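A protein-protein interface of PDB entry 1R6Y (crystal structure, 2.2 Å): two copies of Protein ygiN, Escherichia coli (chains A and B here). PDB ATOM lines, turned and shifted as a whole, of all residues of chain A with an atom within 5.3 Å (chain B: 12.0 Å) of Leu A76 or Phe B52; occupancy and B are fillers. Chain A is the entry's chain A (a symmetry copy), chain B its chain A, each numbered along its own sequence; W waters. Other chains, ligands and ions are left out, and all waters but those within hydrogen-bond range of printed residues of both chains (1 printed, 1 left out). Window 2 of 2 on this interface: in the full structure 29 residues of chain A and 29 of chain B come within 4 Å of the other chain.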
ATOM      1  N   ILE A  69      -7.358  10.492 -12.079  1.00  0.00           N
ATOM      2  CA  ILE A  69      -8.342   9.847 -12.904  1.00  0.00           C
ATOM      3  C   ILE A  69      -8.670  10.637 -14.197  1.00  0.00           C
ATOM      4  O   ILE A  69      -8.939   9.989 -15.262  1.00  0.00           O
ATOM      5  CB  ILE A  69      -9.631   9.569 -12.067  1.00  0.00           C
ATOM      6  CG1 ILE A  69     -10.782   9.067 -12.895  1.00  0.00           C
ATOM      7  CG2 ILE A  69     -10.137  10.848 -11.543  1.00  0.00           C
ATOM      8  CD1 ILE A  69     -10.655   7.588 -13.355  1.00  0.00           C
ATOM      9  N   LEU A  72      -6.019   9.804 -16.876  1.00  0.00           N
ATOM     10  CA  LEU A  72      -6.302   8.464 -17.390  1.00  0.00           C
ATOM     11  C   LEU A  72      -7.514   8.452 -18.279  1.00  0.00           C
ATOM     12  O   LEU A  72      -7.540   7.796 -19.309  1.00  0.00           O
ATOM     13  CB  LEU A  72      -6.616   7.520 -16.235  1.00  0.00           C
ATOM     14  CG  LEU A  72      -6.941   6.066 -16.643  1.00  0.00           C
ATOM     15  CD1 LEU A  72      -5.823   5.527 -17.452  1.00  0.00           C
ATOM     16  CD2 LEU A  72      -7.242   5.174 -15.388  1.00  0.00           C
ATOM     17  N   GLU A  73      -8.592   9.103 -17.861  1.00  0.00           N
ATOM     18  CA  GLU A  73      -9.788   9.154 -18.749  1.00  0.00           C
ATOM     19  C   GLU A  73      -9.474   9.919 -20.125  1.00  0.00           C
ATOM     20  O   GLU A  73      -9.850   9.449 -21.173  1.00  0.00           O
ATOM     21  CB  GLU A  73     -10.986   9.729 -18.040  1.00  0.00           C
ATOM     22  CG  GLU A  73     -11.658   8.697 -17.141  1.00  0.00           C
ATOM     23  CD  GLU A  73     -12.777   9.257 -16.276  1.00  0.00           C
ATOM     24  OE1 GLU A  73     -12.654  10.436 -15.894  1.00  0.00           O
ATOM     25  OE2 GLU A  73     -13.759   8.527 -15.975  1.00  0.00           O
ATOM     26  N   ALA A  74      -8.667  10.984 -20.111  1.00  0.00           N
ATOM     27  CA  ALA A  74      -8.313  11.682 -21.384  1.00  0.00           C
ATOM     28  C   ALA A  74      -7.496  10.759 -22.190  1.00  0.00           C
ATOM     29  O   ALA A  74      -7.627  10.718 -23.385  1.00  0.00           O
ATOM     30  CB  ALA A  74      -7.437  12.934 -21.138  1.00  0.00           C
ATOM     31  N   HIS A  75      -6.594  10.035 -21.531  1.00  0.00           N
ATOM     32  CA  HIS A  75      -5.701   9.085 -22.226  1.00  0.00           C
ATOM     33  C   HIS A  75      -6.477   8.086 -23.085  1.00  0.00           C
ATOM     34  O   HIS A  75      -6.110   7.858 -24.209  1.00  0.00           O
ATOM     35  CB  HIS A  75      -4.769   8.328 -21.219  1.00  0.00           C
ATOM     36  CG  HIS A  75      -4.175   7.072 -21.785  1.00  0.00           C
ATOM     37  ND1 HIS A  75      -4.662   5.820 -21.461  1.00  0.00           N
ATOM     38  CD2 HIS A  75      -3.160   6.874 -22.646  1.00  0.00           C
ATOM     39  CE1 HIS A  75      -3.946   4.904 -22.093  1.00  0.00           C
ATOM     40  NE2 HIS A  75      -3.019   5.510 -22.811  1.00  0.00           N
ATOM     41  N   LEU A  76      -7.587   7.586 -22.565  1.00  0.00           N
ATOM     42  CA  LEU A  76      -8.360   6.565 -23.209  1.00  0.00           C
ATOM     43  C   LEU A  76      -9.123   7.148 -24.417  1.00  0.00           C
ATOM     44  O   LEU A  76      -9.582   6.436 -25.301  1.00  0.00           O
ATOM     45  CB  LEU A  76      -9.370   5.933 -22.210  1.00  0.00           C
ATOM     46  CG  LEU A  76      -8.806   5.095 -21.013  1.00  0.00           C
ATOM     47  CD1 LEU A  76      -9.879   4.769 -19.972  1.00  0.00           C
ATOM     48  CD2 LEU A  76      -8.215   3.848 -21.508  1.00  0.00           C
ATOM     49  N   GLN A  77      -9.352   8.459 -24.421  1.00  0.00           N
ATOM     50  CA  GLN A  77      -9.995   9.080 -25.583  1.00  0.00           C
ATOM     51  C   GLN A  77      -8.993   9.586 -26.612  1.00  0.00           C
ATOM     52  O   GLN A  77      -9.422  10.181 -27.548  1.00  0.00           O
ATOM     53  CB  GLN A  77     -10.895  10.221 -25.125  1.00  0.00           C
ATOM     54  CG  GLN A  77     -12.004   9.808 -24.179  1.00  0.00           C
ATOM     55  CD  GLN A  77     -12.781   8.639 -24.726  1.00  0.00           C
ATOM     56  OE1 GLN A  77     -13.139   7.699 -23.989  1.00  0.00           O
ATOM     57  NE2 GLN A  77     -13.058   8.678 -26.023  1.00  0.00           N
ATOM     58  N   THR A  78      -7.695   9.388 -26.479  1.00  0.00           N
ATOM     59  CA  THR A  78      -6.760   9.961 -27.423  1.00  0.00           C
ATOM     60  C   THR A  78      -6.745   9.181 -28.676  1.00  0.00           C
ATOM     61  O   THR A  78      -7.117   8.006 -28.702  1.00  0.00           O
ATOM     62  CB  THR A  78      -5.307   9.982 -26.946  1.00  0.00           C
ATOM     63  OG1 THR A  78      -4.850   8.633 -26.657  1.00  0.00           O
ATOM     64  CG2 THR A  78      -5.105  10.951 -25.712  1.00  0.00           C
ATOM     65  N   MET A  81      -4.941   5.802 -28.801  1.00  0.00           N
ATOM     66  CA  MET A  81      -5.652   4.664 -28.129  1.00  0.00           C
ATOM     67  C   MET A  81      -6.845   4.103 -28.907  1.00  0.00           C
ATOM     68  O   MET A  81      -7.027   2.888 -29.001  1.00  0.00           O
ATOM     69  CB  MET A  81      -6.035   5.023 -26.740  1.00  0.00           C
ATOM     70  CG  MET A  81      -4.851   5.344 -25.848  1.00  0.00           C
ATOM     71  SD  MET A  81      -3.678   3.982 -25.853  1.00  0.00           S
ATOM     72  CE  MET A  81      -2.631   4.628 -25.867  1.00  0.00           C
ATOM     73  N   LYS A  82      -7.633   4.963 -29.547  1.00  0.00           N
ATOM     74  CA  LYS A  82      -8.699   4.503 -30.419  1.00  0.00           C
ATOM     75  C   LYS A  82      -8.101   3.844 -31.605  1.00  0.00           C
ATOM     76  O   LYS A  82      -8.571   2.843 -32.010  1.00  0.00           O
ATOM     77  CB  LYS A  82      -9.499   5.671 -30.871  1.00  0.00           C
ATOM     78  CG  LYS A  82     -10.300   6.398 -29.707  1.00  0.00           C
ATOM     79  CD  LYS A  82     -11.610   7.093 -30.296  1.00  0.00           C
ATOM     80  CE  LYS A  82     -12.326   8.059 -29.377  1.00  0.00           C
ATOM     81  NZ  LYS A  82     -11.955   9.457 -29.785  1.00  0.00           N
ATOM     82  N   ILE A  97      -8.531  -3.765 -15.571  1.00  0.00           N
ATOM     83  CA  ILE A  97      -7.914  -2.569 -15.139  1.00  0.00           C
ATOM     84  C   ILE A  97      -8.026  -2.385 -13.651  1.00  0.00           C
ATOM     85  O   ILE A  97      -9.118  -2.237 -13.145  1.00  0.00           O
ATOM     86  CB  ILE A  97      -8.508  -1.470 -15.834  1.00  0.00           C
ATOM     87  CG1 ILE A  97      -8.292  -1.614 -17.359  1.00  0.00           C
ATOM     88  CG2 ILE A  97      -7.898  -0.167 -15.400  1.00  0.00           C
ATOM     89  CD1 ILE A  97      -8.984  -0.530 -18.174  1.00  0.00           C
ATOM     90  N   ILE A  99      -6.679   0.120 -10.531  1.00  0.00           N
ATOM     91  CA  ILE A  99      -6.285   1.443 -10.255  1.00  0.00           C
ATOM     92  C   ILE A  99      -5.978   1.427  -8.775  1.00  0.00           C
ATOM     93  O   ILE A  99      -6.874   1.273  -7.946  1.00  0.00           O
ATOM     94  CB  ILE A  99      -7.447   2.465 -10.508  1.00  0.00           C
ATOM     95  CG1 ILE A  99      -8.019   2.318 -11.898  1.00  0.00           C
ATOM     96  CG2 ILE A  99      -6.857   3.942 -10.400  1.00  0.00           C
ATOM     97  CD1 ILE A  99      -9.123   3.373 -12.258  1.00  0.00           C
ATOM     98  N   ASP B  45      -6.431  -1.180  -4.023  1.00  0.00           N
ATOM     99  CA  ASP B  45      -7.369  -0.486  -4.901  1.00  0.00           C
ATOM    100  C   ASP B  45      -7.738   0.896  -4.378  1.00  0.00           C
ATOM    101  O   ASP B  45      -7.845   1.144  -3.154  1.00  0.00           O
ATOM    102  CB  ASP B  45      -8.619  -1.280  -5.211  1.00  0.00           C
ATOM    103  CG  ASP B  45      -8.335  -2.571  -5.850  1.00  0.00           C
ATOM    104  OD1 ASP B  45      -7.682  -2.579  -6.914  1.00  0.00           O
ATOM    105  OD2 ASP B  45      -8.593  -3.714  -5.273  1.00  0.00           O
ATOM    106  N   CYS B  46      -7.766   1.848  -5.295  1.00  0.00           N
ATOM    107  CA  CYS B  46      -8.373   3.147  -5.031  1.00  0.00           C
ATOM    108  C   CYS B  46      -9.793   3.144  -5.704  1.00  0.00           C
ATOM    109  O   CYS B  46      -9.883   3.138  -6.939  1.00  0.00           O
ATOM    110  CB  CYS B  46      -7.473   4.159  -5.662  1.00  0.00           C
ATOM    111  SG  CYS B  46      -8.059   5.839  -5.739  1.00  0.00           S
ATOM    112  N   ALA B  47     -10.868   3.084  -4.943  1.00  0.00           N
ATOM    113  CA  ALA B  47     -12.241   3.178  -5.562  1.00  0.00           C
ATOM    114  C   ALA B  47     -12.376   4.454  -6.427  1.00  0.00           C
ATOM    115  O   ALA B  47     -12.212   5.569  -5.962  1.00  0.00           O
ATOM    116  CB  ALA B  47     -13.320   3.159  -4.586  1.00  0.00           C
ATOM    117  N   ALA B  48     -12.606   4.250  -7.708  1.00  0.00           N
ATOM    118  CA  ALA B  48     -12.607   5.381  -8.576  1.00  0.00           C
ATOM    119  C   ALA B  48     -14.012   5.586  -9.189  1.00  0.00           C
ATOM    120  O   ALA B  48     -14.289   6.645  -9.787  1.00  0.00           O
ATOM    121  CB  ALA B  48     -11.530   5.228  -9.602  1.00  0.00           C
ATOM    122  N   GLY B  49     -14.902   4.605  -9.005  1.00  0.00           N
ATOM    123  CA  GLY B  49     -16.281   4.789  -9.398  1.00  0.00           C
ATOM    124  C   GLY B  49     -16.493   4.725 -10.900  1.00  0.00           C
ATOM    125  O   GLY B  49     -17.528   5.224 -11.400  1.00  0.00           O
ATOM    126  N   VAL B  50     -15.551   4.101 -11.622  1.00  0.00           N
ATOM    127  CA  VAL B  50     -15.573   4.055 -13.063  1.00  0.00           C
ATOM    128  C   VAL B  50     -15.764   2.615 -13.440  1.00  0.00           C
ATOM    129  O   VAL B  50     -15.315   1.689 -12.718  1.00  0.00           O
ATOM    130  CB  VAL B  50     -14.270   4.711 -13.653  1.00  0.00           C
ATOM    131  CG1 VAL B  50     -14.096   6.131 -13.110  1.00  0.00           C
ATOM    132  CG2 VAL B  50     -12.949   3.938 -13.334  1.00  0.00           C
ATOM    133  N   SER B  51     -16.431   2.383 -14.555  1.00  0.00           N
ATOM    134  CA  SER B  51     -17.011   1.090 -14.840  1.00  0.00           C
ATOM    135  C   SER B  51     -16.001   0.137 -15.217  1.00  0.00           C
ATOM    136  O   SER B  51     -16.226  -1.111 -15.078  1.00  0.00           O
ATOM    137  CB  SER B  51     -17.982   1.154 -16.071  1.00  0.00           C
ATOM    138  OG  SER B  51     -17.310   1.557 -17.300  1.00  0.00           O
ATOM    139  N   PHE B  52     -14.924   0.680 -15.799  1.00  0.00           N
ATOM    140  CA  PHE B  52     -13.869  -0.181 -16.306  1.00  0.00           C
ATOM    141  C   PHE B  52     -12.904  -0.702 -15.196  1.00  0.00           C
ATOM    142  O   PHE B  52     -12.113  -1.616 -15.485  1.00  0.00           O
ATOM    143  CB  PHE B  52     -13.059   0.496 -17.482  1.00  0.00           C
ATOM    144  CG  PHE B  52     -12.404   1.814 -17.109  1.00  0.00           C
ATOM    145  CD1 PHE B  52     -11.095   1.830 -16.581  1.00  0.00           C
ATOM    146  CD2 PHE B  52     -13.063   3.015 -17.283  1.00  0.00           C
ATOM    147  CE1 PHE B  52     -10.483   2.965 -16.258  1.00  0.00           C
ATOM    148  CE2 PHE B  52     -12.459   4.219 -16.913  1.00  0.00           C
ATOM    149  CZ  PHE B  52     -11.143   4.197 -16.399  1.00  0.00           C
ATOM    150  N   GLN B  53     -12.939  -0.120 -13.982  1.00  0.00           N
ATOM    151  CA  GLN B  53     -12.053  -0.517 -12.836  1.00  0.00           C
ATOM    152  C   GLN B  53     -12.541  -1.853 -12.229  1.00  0.00           C
ATOM    153  O   GLN B  53     -13.770  -2.018 -11.968  1.00  0.00           O
ATOM    154  CB  GLN B  53     -12.089   0.547 -11.759  1.00  0.00           C
ATOM    155  CG  GLN B  53     -11.274   0.236 -10.596  1.00  0.00           C
ATOM    156  CD  GLN B  53     -11.227   1.290  -9.602  1.00  0.00           C
ATOM    157  OE1 GLN B  53     -12.071   2.178  -9.630  1.00  0.00           O
ATOM    158  NE2 GLN B  53     -10.220   1.225  -8.674  1.00  0.00           N
ATOM    159  N   SER B  54     -11.668  -2.819 -12.036  1.00  0.00           N
ATOM    160  CA  SER B  54     -11.925  -3.936 -11.169  1.00  0.00           C
ATOM    161  C   SER B  54     -11.270  -3.734  -9.788  1.00  0.00           C
ATOM    162  O   SER B  54     -10.098  -3.219  -9.656  1.00  0.00           O
ATOM    163  CB  SER B  54     -11.407  -5.207 -11.709  1.00  0.00           C
ATOM    164  OG  SER B  54     -11.800  -5.282 -13.050  1.00  0.00           O
ATOM    165  N   MET B  55     -12.046  -4.088  -8.773  1.00  0.00           N
ATOM    166  CA  MET B  55     -11.595  -3.909  -7.369  1.00  0.00           C
ATOM    167  C   MET B  55     -11.569  -5.221  -6.658  1.00  0.00           C
ATOM    168  O   MET B  55     -12.345  -6.141  -7.025  1.00  0.00           O
ATOM    169  CB  MET B  55     -12.472  -2.987  -6.690  1.00  0.00           C
ATOM    170  CG  MET B  55     -12.213  -1.680  -7.297  1.00  0.00           C
ATOM    171  SD  MET B  55     -12.810  -0.402  -6.365  1.00  0.00           S
ATOM    172  CE  MET B  55     -11.665  -0.252  -5.335  1.00  0.00           C
ATOM    173  N   ALA B  56     -10.649  -5.327  -5.682  1.00  0.00           N
ATOM    174  CA  ALA B  56     -10.504  -6.524  -4.927  1.00  0.00           C
ATOM    175  C   ALA B  56     -10.076  -6.128  -3.519  1.00  0.00           C
ATOM    176  O   ALA B  56      -8.881  -6.057  -3.180  1.00  0.00           O
ATOM    177  CB  ALA B  56      -9.554  -7.329  -5.574  1.00  0.00           C
HETATM  178  O   HOH W   1     -11.444  -4.006 -15.431  1.00  0.00           O
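The backbone NH (N) of Cys B46 sits at hydrogen-bond distance from the backbone carbonyl oxygen (O) of Ile A99 (2.9 Å).
The backbone NH (N) of Ser B54 sits at hydrogen-bond distance from the backbone carbonyl oxygen (O) of Ile A97 (2.8 Å).
O of Ile A99 lies within hydrogen-bond range of NE2 of Gln B53, at 3.4 Å.
Water W1 lies within hydrogen-bond range of O of Phe B52, OG of Ser B54 and N of Ile A97.
Leu A76 touches just one residue of chain B: Phe B52.
Printed residues of chain A within 4 Å of Phe B52: Leu A76 and Ile A97.
Glu A73 touches one residue of chain B.
No residue of chain B comes within 4 Å of Ala A74.
No residue of chain B comes within 4 Å of His A75.
No residue of chain B comes within 4 Å of Gln A77.
No residue of chain B comes within 4 Å of Thr A78.
No residue of chain B comes within 4 Å of Lys A82.
Ile A97 touches just these residues of chain B: Phe B52, Gln B53 and Ser B54.
Of the printed residues of chain A, Cys B46 touches Ile A99 (2.9 Å).
Of the printed residues of chain A, Ser B54 touches Ile A97 (2.8 Å).
Of the printed residues of chain A, Asp B45 touches Ile A99 (3.6 Å).
Gly B49 touches none of the printed residues of chain A.
Met B55 touches none of the printed residues of chain A.
The nearest residue of chain B that does not touch Leu A76 is Val B50 (7.4 Å).
The nearest printed residue of chain A that does not touch Asp B45 is Ile A97 (6.4 Å).
Among the printed residues, merely in contact across the chains: Ile A69 with Val B50 (3.7 Å), Glu A73 with Val B50 (3.8 Å), Leu A76 with Phe B52 (3.8 Å), Ile A97 with Phe B52 (3.5 Å), Ile A97 with Gln B53 (3.4 Å) and Ile A99 with Asp B45 (3.6 Å).
No position is printed for both chains.
Of the 9 pairs that touch across the chains among the printed residues, none has its exchanged pair printed and touching as well.
O of Cys B46 sits at hydrogen-bond distance from NE2 of Gln B53, at 2.6 Å.
OE1 of Gln B53 sits at hydrogen-bond distance from N of Ala B48, at 2.9 Å.
The backbone NH of Ala B56 is in hydrogen-bond range of the side-chain carboxylate of Asp B45 (2.6 Å).
Of the 12 printed residues of chain B, 6 touch a printed residue of chain A.
Hydrophobic or aromatic side chains of chain B that line the printed part of chain A: Val B50 and Phe B52.
Among the printed residues, no Asp or Glu carboxylate lies within 4 Å of a Lys or Arg side-chain nitrogen of the other chain.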
